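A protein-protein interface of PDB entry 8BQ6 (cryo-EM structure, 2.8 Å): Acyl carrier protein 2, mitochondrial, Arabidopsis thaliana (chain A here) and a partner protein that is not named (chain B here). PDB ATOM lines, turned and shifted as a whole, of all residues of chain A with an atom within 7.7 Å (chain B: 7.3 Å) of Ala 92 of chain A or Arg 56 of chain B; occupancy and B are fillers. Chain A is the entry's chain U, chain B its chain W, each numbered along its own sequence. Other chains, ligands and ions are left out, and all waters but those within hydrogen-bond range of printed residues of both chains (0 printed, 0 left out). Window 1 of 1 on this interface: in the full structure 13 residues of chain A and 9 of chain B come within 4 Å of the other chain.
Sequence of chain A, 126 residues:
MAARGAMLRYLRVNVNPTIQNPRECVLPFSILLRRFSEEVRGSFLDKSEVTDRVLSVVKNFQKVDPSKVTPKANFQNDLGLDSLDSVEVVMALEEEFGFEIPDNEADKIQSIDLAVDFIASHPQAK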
ATOM      1  N   ARG A  53       6.941  -4.613  20.994  1.00  0.00           N
ATOM      2  CA  ARG A  53       6.080  -5.092  22.108  1.00  0.00           C
ATOM      3  C   ARG A  53       5.279  -6.276  21.593  1.00  0.00           C
ATOM      4  O   ARG A  53       5.094  -7.226  22.366  1.00  0.00           O
ATOM      5  CB  ARG A  53       5.158  -3.983  22.611  1.00  0.00           C
ATOM      6  CG  ARG A  53       5.731  -3.124  23.729  1.00  0.00           C
ATOM      7  CD  ARG A  53       4.945  -1.830  23.817  1.00  0.00           C
ATOM      8  NE  ARG A  53       5.027  -1.134  25.091  1.00  0.00           N
ATOM      9  CZ  ARG A  53       4.040  -1.032  25.977  1.00  0.00           C
ATOM     10  NH1 ARG A  53       2.866  -1.594  25.749  1.00  0.00           N
ATOM     11  NH2 ARG A  53       4.234  -0.370  27.103  1.00  0.00           N
ATOM     12  N   VAL A  57       5.962 -10.437  22.944  1.00  0.00           N
ATOM     13  CA  VAL A  57       4.861 -11.286  23.501  1.00  0.00           C
ATOM     14  C   VAL A  57       4.667 -12.546  22.657  1.00  0.00           C
ATOM     15  O   VAL A  57       4.267 -13.556  23.249  1.00  0.00           O
ATOM     16  CB  VAL A  57       3.536 -10.512  23.675  1.00  0.00           C
ATOM     17  CG1 VAL A  57       3.665  -9.378  24.680  1.00  0.00           C
ATOM     18  CG2 VAL A  57       2.970 -10.007  22.360  1.00  0.00           C
ATOM     19  N   VAL A  58       4.948 -12.501  21.352  1.00  0.00           N
ATOM     20  CA  VAL A  58       4.844 -13.763  20.564  1.00  0.00           C
ATOM     21  C   VAL A  58       6.062 -14.647  20.880  1.00  0.00           C
ATOM     22  O   VAL A  58       5.859 -15.853  21.066  1.00  0.00           O
ATOM     23  CB  VAL A  58       4.635 -13.526  19.052  1.00  0.00           C
ATOM     24  CG1 VAL A  58       3.230 -13.036  18.748  1.00  0.00           C
ATOM     25  CG2 VAL A  58       5.663 -12.600  18.436  1.00  0.00           C
ATOM     26  N   PHE A  61       5.487 -16.070  24.262  1.00  0.00           N
ATOM     27  CA  PHE A  61       4.411 -17.087  24.146  1.00  0.00           C
ATOM     28  C   PHE A  61       5.042 -18.442  23.821  1.00  0.00           C
ATOM     29  O   PHE A  61       5.952 -18.497  22.967  1.00  0.00           O
ATOM     30  CB  PHE A  61       3.402 -16.667  23.075  1.00  0.00           C
ATOM     31  CG  PHE A  61       2.098 -17.421  23.069  1.00  0.00           C
ATOM     32  CD1 PHE A  61       1.222 -17.332  24.137  1.00  0.00           C
ATOM     33  CD2 PHE A  61       1.737 -18.204  21.984  1.00  0.00           C
ATOM     34  CE1 PHE A  61       0.019 -18.017  24.124  1.00  0.00           C
ATOM     35  CE2 PHE A  61       0.534 -18.888  21.971  1.00  0.00           C
ATOM     36  CZ  PHE A  61      -0.322 -18.796  23.042  1.00  0.00           C
ATOM     37  N   SER A  86      -3.826 -19.182  18.490  1.00  0.00           N
ATOM     38  CA  SER A  86      -3.970 -17.853  17.836  1.00  0.00           C
ATOM     39  C   SER A  86      -4.896 -16.949  18.659  1.00  0.00           C
ATOM     40  O   SER A  86      -4.575 -15.752  18.787  1.00  0.00           O
ATOM     41  CB  SER A  86      -4.459 -18.001  16.418  1.00  0.00           C
ATOM     42  OG  SER A  86      -3.551 -18.775  15.647  1.00  0.00           O
ATOM     43  N   VAL A  87      -5.996 -17.497  19.190  1.00  0.00           N
ATOM     44  CA  VAL A  87      -6.921 -16.707  20.059  1.00  0.00           C
ATOM     45  C   VAL A  87      -6.139 -16.209  21.281  1.00  0.00           C
ATOM     46  O   VAL A  87      -6.240 -15.005  21.587  1.00  0.00           O
ATOM     47  CB  VAL A  87      -8.156 -17.538  20.463  1.00  0.00           C
ATOM     48  CG1 VAL A  87      -9.002 -16.847  21.522  1.00  0.00           C
ATOM     49  CG2 VAL A  87      -9.011 -17.888  19.256  1.00  0.00           C
ATOM     50  N   GLU A  88      -5.300 -17.049  21.883  1.00  0.00           N
ATOM     51  CA  GLU A  88      -4.531 -16.651  23.096  1.00  0.00           C
ATOM     52  C   GLU A  88      -3.557 -15.497  22.804  1.00  0.00           C
ATOM     53  O   GLU A  88      -3.194 -14.790  23.767  1.00  0.00           O
ATOM     54  CB  GLU A  88      -3.795 -17.870  23.651  1.00  0.00           C
ATOM     55  CG  GLU A  88      -3.940 -18.034  25.151  1.00  0.00           C
ATOM     56  CD  GLU A  88      -3.109 -19.150  25.762  1.00  0.00           C
ATOM     57  OE1 GLU A  88      -3.037 -20.236  25.152  1.00  0.00           O
ATOM     58  OE2 GLU A  88      -2.537 -18.928  26.848  1.00  0.00           O
ATOM     59  N   VAL A  89      -3.149 -15.295  21.544  1.00  0.00           N
ATOM     60  CA  VAL A  89      -2.136 -14.240  21.214  1.00  0.00           C
ATOM     61  C   VAL A  89      -2.810 -12.861  21.215  1.00  0.00           C
ATOM     62  O   VAL A  89      -2.279 -11.956  21.869  1.00  0.00           O
ATOM     63  CB  VAL A  89      -1.416 -14.526  19.878  1.00  0.00           C
ATOM     64  CG1 VAL A  89      -0.630 -13.328  19.370  1.00  0.00           C
ATOM     65  CG2 VAL A  89      -0.518 -15.748  19.972  1.00  0.00           C
ATOM     66  N   VAL A  90      -3.936 -12.710  20.513  1.00  0.00           N
ATOM     67  CA  VAL A  90      -4.676 -11.409  20.526  1.00  0.00           C
ATOM     68  C   VAL A  90      -5.012 -11.051  21.978  1.00  0.00           C
ATOM     69  O   VAL A  90      -4.846  -9.874  22.329  1.00  0.00           O
ATOM     70  CB  VAL A  90      -5.931 -11.456  19.637  1.00  0.00           C
ATOM     71  CG1 VAL A  90      -6.483 -10.070  19.352  1.00  0.00           C
ATOM     72  CG2 VAL A  90      -5.677 -12.208  18.340  1.00  0.00           C
ATOM     73  N   MET A  91      -5.439 -12.028  22.791  1.00  0.00           N
ATOM     74  CA  MET A  91      -5.719 -11.791  24.234  1.00  0.00           C
ATOM     75  C   MET A  91      -4.489 -11.169  24.907  1.00  0.00           C
ATOM     76  O   MET A  91      -4.651 -10.150  25.597  1.00  0.00           O
ATOM     77  CB  MET A  91      -6.049 -13.104  24.953  1.00  0.00           C
ATOM     78  CG  MET A  91      -7.355 -13.745  24.528  1.00  0.00           C
ATOM     79  SD  MET A  91      -8.691 -12.552  24.296  1.00  0.00           S
ATOM     80  CE  MET A  91      -9.085 -12.154  25.997  1.00  0.00           C
ATOM     81  N   ALA A  92      -3.308 -11.772  24.721  1.00  0.00           N
ATOM     82  CA  ALA A  92      -2.058 -11.257  25.332  1.00  0.00           C
ATOM     83  C   ALA A  92      -1.792  -9.802  24.920  1.00  0.00           C
ATOM     84  O   ALA A  92      -1.373  -9.031  25.801  1.00  0.00           O
ATOM     85  CB  ALA A  92      -0.907 -12.162  24.972  1.00  0.00           C
ATOM     86  N   LEU A  93      -2.028  -9.441  23.652  1.00  0.00           N
ATOM     87  CA  LEU A  93      -1.814  -8.047  23.161  1.00  0.00           C
ATOM     88  C   LEU A  93      -2.834  -7.112  23.809  1.00  0.00           C
ATOM     89  O   LEU A  93      -2.435  -6.024  24.203  1.00  0.00           O
ATOM     90  CB  LEU A  93      -1.963  -8.034  21.639  1.00  0.00           C
ATOM     91  CG  LEU A  93      -0.906  -8.813  20.867  1.00  0.00           C
ATOM     92  CD1 LEU A  93      -1.437  -9.236  19.507  1.00  0.00           C
ATOM     93  CD2 LEU A  93       0.337  -7.965  20.706  1.00  0.00           C
ATOM     94  N   GLU A  94      -4.103  -7.512  23.886  1.00  0.00           N
ATOM     95  CA  GLU A  94      -5.140  -6.715  24.596  1.00  0.00           C
ATOM     96  C   GLU A  94      -4.622  -6.327  25.979  1.00  0.00           C
ATOM     97  O   GLU A  94      -4.585  -5.127  26.265  1.00  0.00           O
ATOM     98  CB  GLU A  94      -6.400  -7.549  24.800  1.00  0.00           C
ATOM     99  CG  GLU A  94      -7.322  -7.593  23.604  1.00  0.00           C
ATOM    100  CD  GLU A  94      -8.276  -8.772  23.574  1.00  0.00           C
ATOM    101  OE1 GLU A  94      -9.070  -8.914  24.526  1.00  0.00           O
ATOM    102  OE2 GLU A  94      -8.226  -9.543  22.595  1.00  0.00           O
ATOM    103  N   GLU A  95      -4.241  -7.317  26.794  1.00  0.00           N
ATOM    104  CA  GLU A  95      -3.694  -7.057  28.154  1.00  0.00           C
ATOM    105  C   GLU A  95      -2.460  -6.151  28.066  1.00  0.00           C
ATOM    106  O   GLU A  95      -2.414  -5.155  28.812  1.00  0.00           O
ATOM    107  CB  GLU A  95      -3.358  -8.391  28.823  1.00  0.00           C
ATOM    108  CG  GLU A  95      -2.529  -8.277  30.086  1.00  0.00           C
ATOM    109  CD  GLU A  95      -1.182  -8.972  29.999  1.00  0.00           C
ATOM    110  OE1 GLU A  95      -1.111 -10.045  29.368  1.00  0.00           O
ATOM    111  OE2 GLU A  95      -0.206  -8.432  30.556  1.00  0.00           O
ATOM    112  N   GLU A  96      -1.517  -6.461  27.178  1.00  0.00           N
ATOM    113  CA  GLU A  96      -0.280  -5.644  27.029  1.00  0.00           C
ATOM    114  C   GLU A  96      -0.637  -4.170  26.834  1.00  0.00           C
ATOM    115  O   GLU A  96      -0.081  -3.330  27.565  1.00  0.00           O
ATOM    116  CB  GLU A  96       0.558  -6.159  25.857  1.00  0.00           C
ATOM    117  CG  GLU A  96       1.593  -5.173  25.341  1.00  0.00           C
ATOM    118  CD  GLU A  96       2.930  -5.161  26.057  1.00  0.00           C
ATOM    119  OE1 GLU A  96       3.856  -5.852  25.589  1.00  0.00           O
ATOM    120  OE2 GLU A  96       3.048  -4.446  27.070  1.00  0.00           O
ATOM    121  N   PHE A  97      -1.525  -3.869  25.889  1.00  0.00           N
ATOM    122  CA  PHE A  97      -1.817  -2.447  25.580  1.00  0.00           C
ATOM    123  C   PHE A  97      -3.010  -1.972  26.411  1.00  0.00           C
ATOM    124  O   PHE A  97      -3.462  -0.843  26.181  1.00  0.00           O
ATOM    125  CB  PHE A  97      -1.936  -2.275  24.064  1.00  0.00           C
ATOM    126  CG  PHE A  97      -0.653  -2.530  23.319  1.00  0.00           C
ATOM    127  CD1 PHE A  97       0.354  -1.582  23.303  1.00  0.00           C
ATOM    128  CD2 PHE A  97      -0.443  -3.724  22.647  1.00  0.00           C
ATOM    129  CE1 PHE A  97       1.534  -1.814  22.614  1.00  0.00           C
ATOM    130  CE2 PHE A  97       0.739  -3.958  21.965  1.00  0.00           C
ATOM    131  CZ  PHE A  97       1.725  -3.002  21.950  1.00  0.00           C
ATOM    132  N   GLY A  98      -3.532  -2.817  27.307  1.00  0.00           N
ATOM    133  CA  GLY A  98      -4.569  -2.339  28.246  1.00  0.00           C
ATOM    134  C   GLY A  98      -5.912  -1.998  27.625  1.00  0.00           C
ATOM    135  O   GLY A  98      -6.662  -1.245  28.278  1.00  0.00           O
ATOM    136  N   ILE A 101     -10.173  -5.539  22.272  1.00  0.00           N
ATOM    137  CA  ILE A 101     -10.131  -5.591  20.781  1.00  0.00           C
ATOM    138  C   ILE A 101     -11.411  -6.291  20.333  1.00  0.00           C
ATOM    139  O   ILE A 101     -11.649  -7.426  20.789  1.00  0.00           O
ATOM    140  CB  ILE A 101      -8.856  -6.297  20.276  1.00  0.00           C
ATOM    141  CG1 ILE A 101      -7.591  -5.525  20.663  1.00  0.00           C
ATOM    142  CG2 ILE A 101      -8.919  -6.549  18.777  1.00  0.00           C
ATOM    143  CD1 ILE A 101      -6.301  -6.224  20.304  1.00  0.00           C
ATOM    144  N   PHE B  30     -13.746 -18.952  26.165  1.00  0.00           N
ATOM    145  CA  PHE B  30     -12.351 -18.739  26.538  1.00  0.00           C
ATOM    146  C   PHE B  30     -12.029 -17.258  26.616  1.00  0.00           C
ATOM    147  O   PHE B  30     -11.257 -16.821  27.477  1.00  0.00           O
ATOM    148  CB  PHE B  30     -11.431 -19.423  25.529  1.00  0.00           C
ATOM    149  CG  PHE B  30      -9.973 -19.219  25.806  1.00  0.00           C
ATOM    150  CD1 PHE B  30      -9.418 -19.648  26.996  1.00  0.00           C
ATOM    151  CD2 PHE B  30      -9.159 -18.582  24.884  1.00  0.00           C
ATOM    152  CE1 PHE B  30      -8.075 -19.463  27.258  1.00  0.00           C
ATOM    153  CE2 PHE B  30      -7.816 -18.391  25.142  1.00  0.00           C
ATOM    154  CZ  PHE B  30      -7.274 -18.832  26.331  1.00  0.00           C
ATOM    155  N   ALA B  33     -13.627 -15.980  29.853  1.00  0.00           N
ATOM    156  CA  ALA B  33     -12.858 -16.445  31.001  1.00  0.00           C
ATOM    157  C   ALA B  33     -11.563 -15.660  31.150  1.00  0.00           C
ATOM    158  O   ALA B  33     -11.198 -15.257  32.260  1.00  0.00           O
ATOM    159  CB  ALA B  33     -12.574 -17.941  30.872  1.00  0.00           C
ATOM    160  N   CYS B  34     -10.864 -15.414  30.040  1.00  0.00           N
ATOM    161  CA  CYS B  34      -9.607 -14.680  30.109  1.00  0.00           C
ATOM    162  C   CYS B  34      -9.837 -13.214  30.458  1.00  0.00           C
ATOM    163  O   CYS B  34      -9.032 -12.609  31.175  1.00  0.00           O
ATOM    164  CB  CYS B  34      -8.851 -14.801  28.789  1.00  0.00           C
ATOM    165  SG  CYS B  34      -7.258 -13.960  28.801  1.00  0.00           S
ATOM    166  N   ARG B  35     -10.920 -12.618  29.961  1.00  0.00           N
ATOM    167  CA  ARG B  35     -11.132 -11.158  30.183  1.00  0.00           C
ATOM    168  C   ARG B  35     -11.461 -10.872  31.656  1.00  0.00           C
ATOM    169  O   ARG B  35     -11.267  -9.719  32.072  1.00  0.00           O
ATOM    170  CB  ARG B  35     -12.194 -10.608  29.227  1.00  0.00           C
ATOM    171  CG  ARG B  35     -11.629 -10.155  27.889  1.00  0.00           C
ATOM    172  CD  ARG B  35     -12.682  -9.944  26.819  1.00  0.00           C
ATOM    173  NE  ARG B  35     -12.110  -9.339  25.625  1.00  0.00           N
ATOM    174  CZ  ARG B  35     -12.545  -9.539  24.387  1.00  0.00           C
ATOM    175  NH1 ARG B  35     -13.576 -10.335  24.165  1.00  0.00           N
ATOM    176  NH2 ARG B  35     -11.948  -8.939  23.373  1.00  0.00           N
ATOM    177  N   ILE B  37      -9.866 -12.282  34.129  1.00  0.00           N
ATOM    178  CA  ILE B  37      -8.685 -12.589  34.939  1.00  0.00           C
ATOM    179  C   ILE B  37      -8.272 -11.431  35.841  1.00  0.00           C
ATOM    180  O   ILE B  37      -7.971 -11.676  37.020  1.00  0.00           O
ATOM    181  CB  ILE B  37      -7.539 -13.076  34.034  1.00  0.00           C
ATOM    182  CG1 ILE B  37      -7.684 -14.572  33.778  1.00  0.00           C
ATOM    183  CG2 ILE B  37      -6.187 -12.757  34.650  1.00  0.00           C
ATOM    184  CD1 ILE B  37      -6.787 -15.080  32.698  1.00  0.00           C
ATOM    185  N   PRO B  38      -8.215 -10.176  35.372  1.00  0.00           N
ATOM    186  CA  PRO B  38      -7.861  -9.090  36.303  1.00  0.00           C
ATOM    187  C   PRO B  38      -8.813  -8.973  37.478  1.00  0.00           C
ATOM    188  O   PRO B  38      -8.378  -8.675  38.598  1.00  0.00           O
ATOM    189  CB  PRO B  38      -7.905  -7.841  35.413  1.00  0.00           C
ATOM    190  CG  PRO B  38      -7.729  -8.352  34.036  1.00  0.00           C
ATOM    191  CD  PRO B  38      -8.430  -9.661  34.008  1.00  0.00           C
ATOM    192  N   ALA B  51       1.086 -15.430  38.313  1.00  0.00           N
ATOM    193  CA  ALA B  51       1.006 -14.512  37.192  1.00  0.00           C
ATOM    194  C   ALA B  51      -0.325 -14.673  36.455  1.00  0.00           C
ATOM    195  O   ALA B  51      -0.913 -15.757  36.449  1.00  0.00           O
ATOM    196  CB  ALA B  51       2.163 -14.752  36.230  1.00  0.00           C
ATOM    197  N   PRO B  52      -0.816 -13.600  35.826  1.00  0.00           N
ATOM    198  CA  PRO B  52      -2.053 -13.716  35.031  1.00  0.00           C
ATOM    199  C   PRO B  52      -1.962 -14.715  33.894  1.00  0.00           C
ATOM    200  O   PRO B  52      -2.978 -15.324  33.538  1.00  0.00           O
ATOM    201  CB  PRO B  52      -2.273 -12.290  34.503  1.00  0.00           C
ATOM    202  CG  PRO B  52      -1.407 -11.408  35.339  1.00  0.00           C
ATOM    203  CD  PRO B  52      -0.274 -12.233  35.833  1.00  0.00           C
ATOM    204  N   SER B  53      -0.783 -14.889  33.290  1.00  0.00           N
ATOM    205  CA  SER B  53      -0.650 -15.869  32.218  1.00  0.00           C
ATOM    206  C   SER B  53      -0.815 -17.287  32.741  1.00  0.00           C
ATOM    207  O   SER B  53      -1.340 -18.154  32.033  1.00  0.00           O
ATOM    208  CB  SER B  53       0.703 -15.712  31.525  1.00  0.00           C
ATOM    209  OG  SER B  53       1.707 -15.342  32.453  1.00  0.00           O
ATOM    210  N   GLN B  54      -0.362 -17.544  33.969  1.00  0.00           N
ATOM    211  CA  GLN B  54      -0.578 -18.849  34.582  1.00  0.00           C
ATOM    212  C   GLN B  54      -2.060 -19.147  34.730  1.00  0.00           C
ATOM    213  O   GLN B  54      -2.490 -20.297  34.584  1.00  0.00           O
ATOM    214  CB  GLN B  54       0.112 -18.909  35.940  1.00  0.00           C
ATOM    215  CG  GLN B  54       1.535 -18.425  35.924  1.00  0.00           C
ATOM    216  CD  GLN B  54       2.333 -18.947  37.099  1.00  0.00           C
ATOM    217  OE1 GLN B  54       2.117 -18.571  38.219  1.00  0.00           O
ATOM    218  NE2 GLN B  54       3.252 -19.846  36.830  1.00  0.00           N
ATOM    219  N   LEU B  55      -2.853 -18.124  35.049  1.00  0.00           N
ATOM    220  CA  LEU B  55      -4.301 -18.279  35.038  1.00  0.00           C
ATOM    221  C   LEU B  55      -4.798 -18.600  33.635  1.00  0.00           C
ATOM    222  O   LEU B  55      -5.667 -19.458  33.450  1.00  0.00           O
ATOM    223  CB  LEU B  55      -4.964 -17.011  35.572  1.00  0.00           C
ATOM    224  CG  LEU B  55      -4.812 -16.763  37.073  1.00  0.00           C
ATOM    225  CD1 LEU B  55      -5.864 -15.780  37.540  1.00  0.00           C
ATOM    226  CD2 LEU B  55      -4.912 -18.069  37.851  1.00  0.00           C
ATOM    227  N   ARG B  56      -4.239 -17.906  32.640  1.00  0.00           N
ATOM    228  CA  ARG B  56      -4.607 -18.165  31.223  1.00  0.00           C
ATOM    229  C   ARG B  56      -4.211 -19.592  30.836  1.00  0.00           C
ATOM    230  O   ARG B  56      -5.002 -20.230  30.125  1.00  0.00           O
ATOM    231  CB  ARG B  56      -3.900 -17.151  30.323  1.00  0.00           C
ATOM    232  CG  ARG B  56      -4.685 -16.685  29.108  1.00  0.00           C
ATOM    233  CD  ARG B  56      -3.949 -15.505  28.498  1.00  0.00           C
ATOM    234  NE  ARG B  56      -3.896 -14.382  29.428  1.00  0.00           N
ATOM    235  CZ  ARG B  56      -3.026 -13.380  29.374  1.00  0.00           C
ATOM    236  NH1 ARG B  56      -2.108 -13.341  28.423  1.00  0.00           N
ATOM    237  NH2 ARG B  56      -3.075 -12.416  30.276  1.00  0.00           N
ATOM    238  N   TYR B  57      -3.035 -20.070  31.268  1.00  0.00           N
ATOM    239  CA  TYR B  57      -2.577 -21.397  30.876  1.00  0.00           C
ATOM    240  C   TYR B  57      -3.488 -22.478  31.437  1.00  0.00           C
ATOM    241  O   TYR B  57      -3.811 -23.447  30.741  1.00  0.00           O
ATOM    242  CB  TYR B  57      -1.132 -21.611  31.326  1.00  0.00           C
ATOM    243  CG  TYR B  57      -0.768 -23.053  31.608  1.00  0.00           C
ATOM    244  CD1 TYR B  57      -0.936 -23.608  32.873  1.00  0.00           C
ATOM    245  CD2 TYR B  57      -0.269 -23.863  30.599  1.00  0.00           C
ATOM    246  CE1 TYR B  57      -0.607 -24.929  33.122  1.00  0.00           C
ATOM    247  CE2 TYR B  57       0.062 -25.179  30.839  1.00  0.00           C
ATOM    248  CZ  TYR B  57      -0.107 -25.707  32.099  1.00  0.00           C
ATOM    249  OH  TYR B  57       0.224 -27.023  32.330  1.00  0.00           O
ATOM    250  N   ALA B  58      -3.927 -22.289  32.685  1.00  0.00           N
ATOM    251  CA  ALA B  58      -4.820 -23.274  33.337  1.00  0.00           C
ATOM    252  C   ALA B  58      -6.150 -23.342  32.585  1.00  0.00           C
ATOM    253  O   ALA B  58      -6.690 -24.449  32.461  1.00  0.00           O
ATOM    254  CB  ALA B  58      -5.027 -22.910  34.785  1.00  0.00           C
ATOM    255  N   ILE B  59      -6.652 -22.201  32.111  1.00  0.00           N
ATOM    256  CA  ILE B  59      -7.905 -22.187  31.363  1.00  0.00           C
ATOM    257  C   ILE B  59      -7.722 -22.863  30.011  1.00  0.00           C
ATOM    258  O   ILE B  59      -8.526 -23.713  29.610  1.00  0.00           O
ATOM    259  CB  ILE B  59      -8.433 -20.750  31.219  1.00  0.00           C
ATOM    260  CG1 ILE B  59      -8.717 -20.163  32.600  1.00  0.00           C
ATOM    261  CG2 ILE B  59      -9.691 -20.735  30.371  1.00  0.00           C
ATOM    262  CD1 ILE B  59      -9.123 -18.713  32.583  1.00  0.00           C
ATOM    263  N   SER B  60      -6.649 -22.514  29.296  1.00  0.00           N
ATOM    264  CA  SER B  60      -6.402 -23.149  28.005  1.00  0.00           C
ATOM    265  C   SER B  60      -6.049 -24.619  28.177  1.00  0.00           C
ATOM    266  O   SER B  60      -6.411 -25.447  27.333  1.00  0.00           O
ATOM    267  CB  SER B  60      -5.292 -22.424  27.249  1.00  0.00           C
ATOM    268  OG  SER B  60      -4.240 -22.062  28.121  1.00  0.00           O
ATOM    269  N   ALA B  61      -5.334 -24.964  29.252  1.00  0.00           N
ATOM    270  CA  ALA B  61      -5.110 -26.375  29.541  1.00  0.00           C
ATOM    271  C   ALA B  61      -6.432 -27.109  29.630  1.00  0.00           C
ATOM    272  O   ALA B  61      -6.683 -28.032  28.850  1.00  0.00           O
ATOM    273  CB  ALA B  61      -4.325 -26.547  30.842  1.00  0.00           C
ATOM    274  N   GLN B  62      -7.284 -26.674  30.566  1.00  0.00           N
ATOM    275  CA  GLN B  62      -8.636 -27.270  30.738  1.00  0.00           C
ATOM    276  C   GLN B  62      -9.284 -27.525  29.379  1.00  0.00           C
ATOM    277  O   GLN B  62      -9.819 -28.633  29.184  1.00  0.00           O
ATOM    278  CB  GLN B  62      -9.512 -26.301  31.527  1.00  0.00           C
ATOM    279  CG  GLN B  62      -9.372 -26.427  33.033  1.00  0.00           C
ATOM    280  CD  GLN B  62      -9.832 -27.775  33.526  1.00  0.00           C
ATOM    281  OE1 GLN B  62     -10.971 -28.183  33.303  1.00  0.00           O
ATOM    282  NE2 GLN B  62      -8.941 -28.481  34.201  1.00  0.00           N
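NH2 of Arg 35 of chain B is in salt-bridge range of OE1 of Glu 94 of chain A (3.1 Å). The guanidinium group (NH2) of Arg 35 of chain B sits at hydrogen-bond distance from the backbone carbonyl oxygen (O) of Ile 101 of chain A (3.0 Å). The guanidinium group (NH2) of Arg 56 of chain B is in salt-bridge range of the side-chain carboxylate (OE1) of Glu 95 of chain A.
Among the printed residues, merely in contact across the chains: Glu 88 of chain A with Phe 30 of chain B, Glu 88 of chain A with Ser 60 of chain B, Ala 92 of chain A with Arg 56 of chain B, Met 91 of chain A with Arg 35 of chain B, Val 87 of chain A with Phe 30 of chain B, Met 91 of chain A with Cys 34 of chain B and Glu 88 of chain A with Arg 56 of chain B.
Printed residues of chain B within 4 Å of Val 87 of chain A: Phe 30. Ala 92 of chain A touches one residue of chain B. Of the printed residues of chain B, Glu 94 of chain A touches Arg 35 (3.1 Å). Printed residues of chain B within 4 Å of Glu 95 of chain A: Arg 56. Printed residues of chain A within 4 Å of Phe 30 of chain B: Val 87 (3.8 Å) and Glu 88 (3.6 Å). Of the printed residues of chain A, Cys 34 of chain B touches Met 91. Of chain A, only Glu 88, Ala 92 and Glu 95 come within 4 Å of Arg 56 of chain B. The nearest residue of chain B that does not touch Ala 92 of chain A is Cys 34 of chain B (6.1 Å). The nearest residue of chain A that does not touch Arg 56 of chain B is Met 91 of chain A (4.8 Å). The nearest printed residue of chain A that does not touch Phe 30 of chain B is Met 91 of chain A (4.7 Å).
Of the 18 printed residues of chain A, 7 touch a printed residue of chain B. Hydrophobic or aromatic side chains of chain A within 4 Å of the printed part of chain B: Val 87, Met 91 and Ala 92. Of the 18 printed residues of chain B, 5 touch a printed residue of chain A. Printed residues of chain B that touch a printed residue of chain A: Phe 30, Cys 34, Arg 35, Arg 56 and Ser 60. Hydrophobic or aromatic side chains of chain B within 4 Å of the printed part of chain A: Phe 30. Among the printed residues, 10 pairs touch across the chains. Among the printed residues, Asp or Glu carboxylates within 4 Å of a Lys or Arg side-chain nitrogen of the other chain: Glu 94 of chain A with Arg 35 of chain B (3.1 Å) and Glu 95 of chain A with Arg 56 of chain B (3.2 Å).
The backbone carbonyl oxygen of Tyr 57 of chain B lies within hydrogen-bond range of the side-chain hydroxyl of Ser 60 of chain B. NE of Arg 56 of chain B lies within hydrogen-bond range of SG of Cys 34 of chain B (3.4 Å). OG of Ser 60 of chain B sits at hydrogen-bond distance from O of Arg 56 of chain B (2.8 Å).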
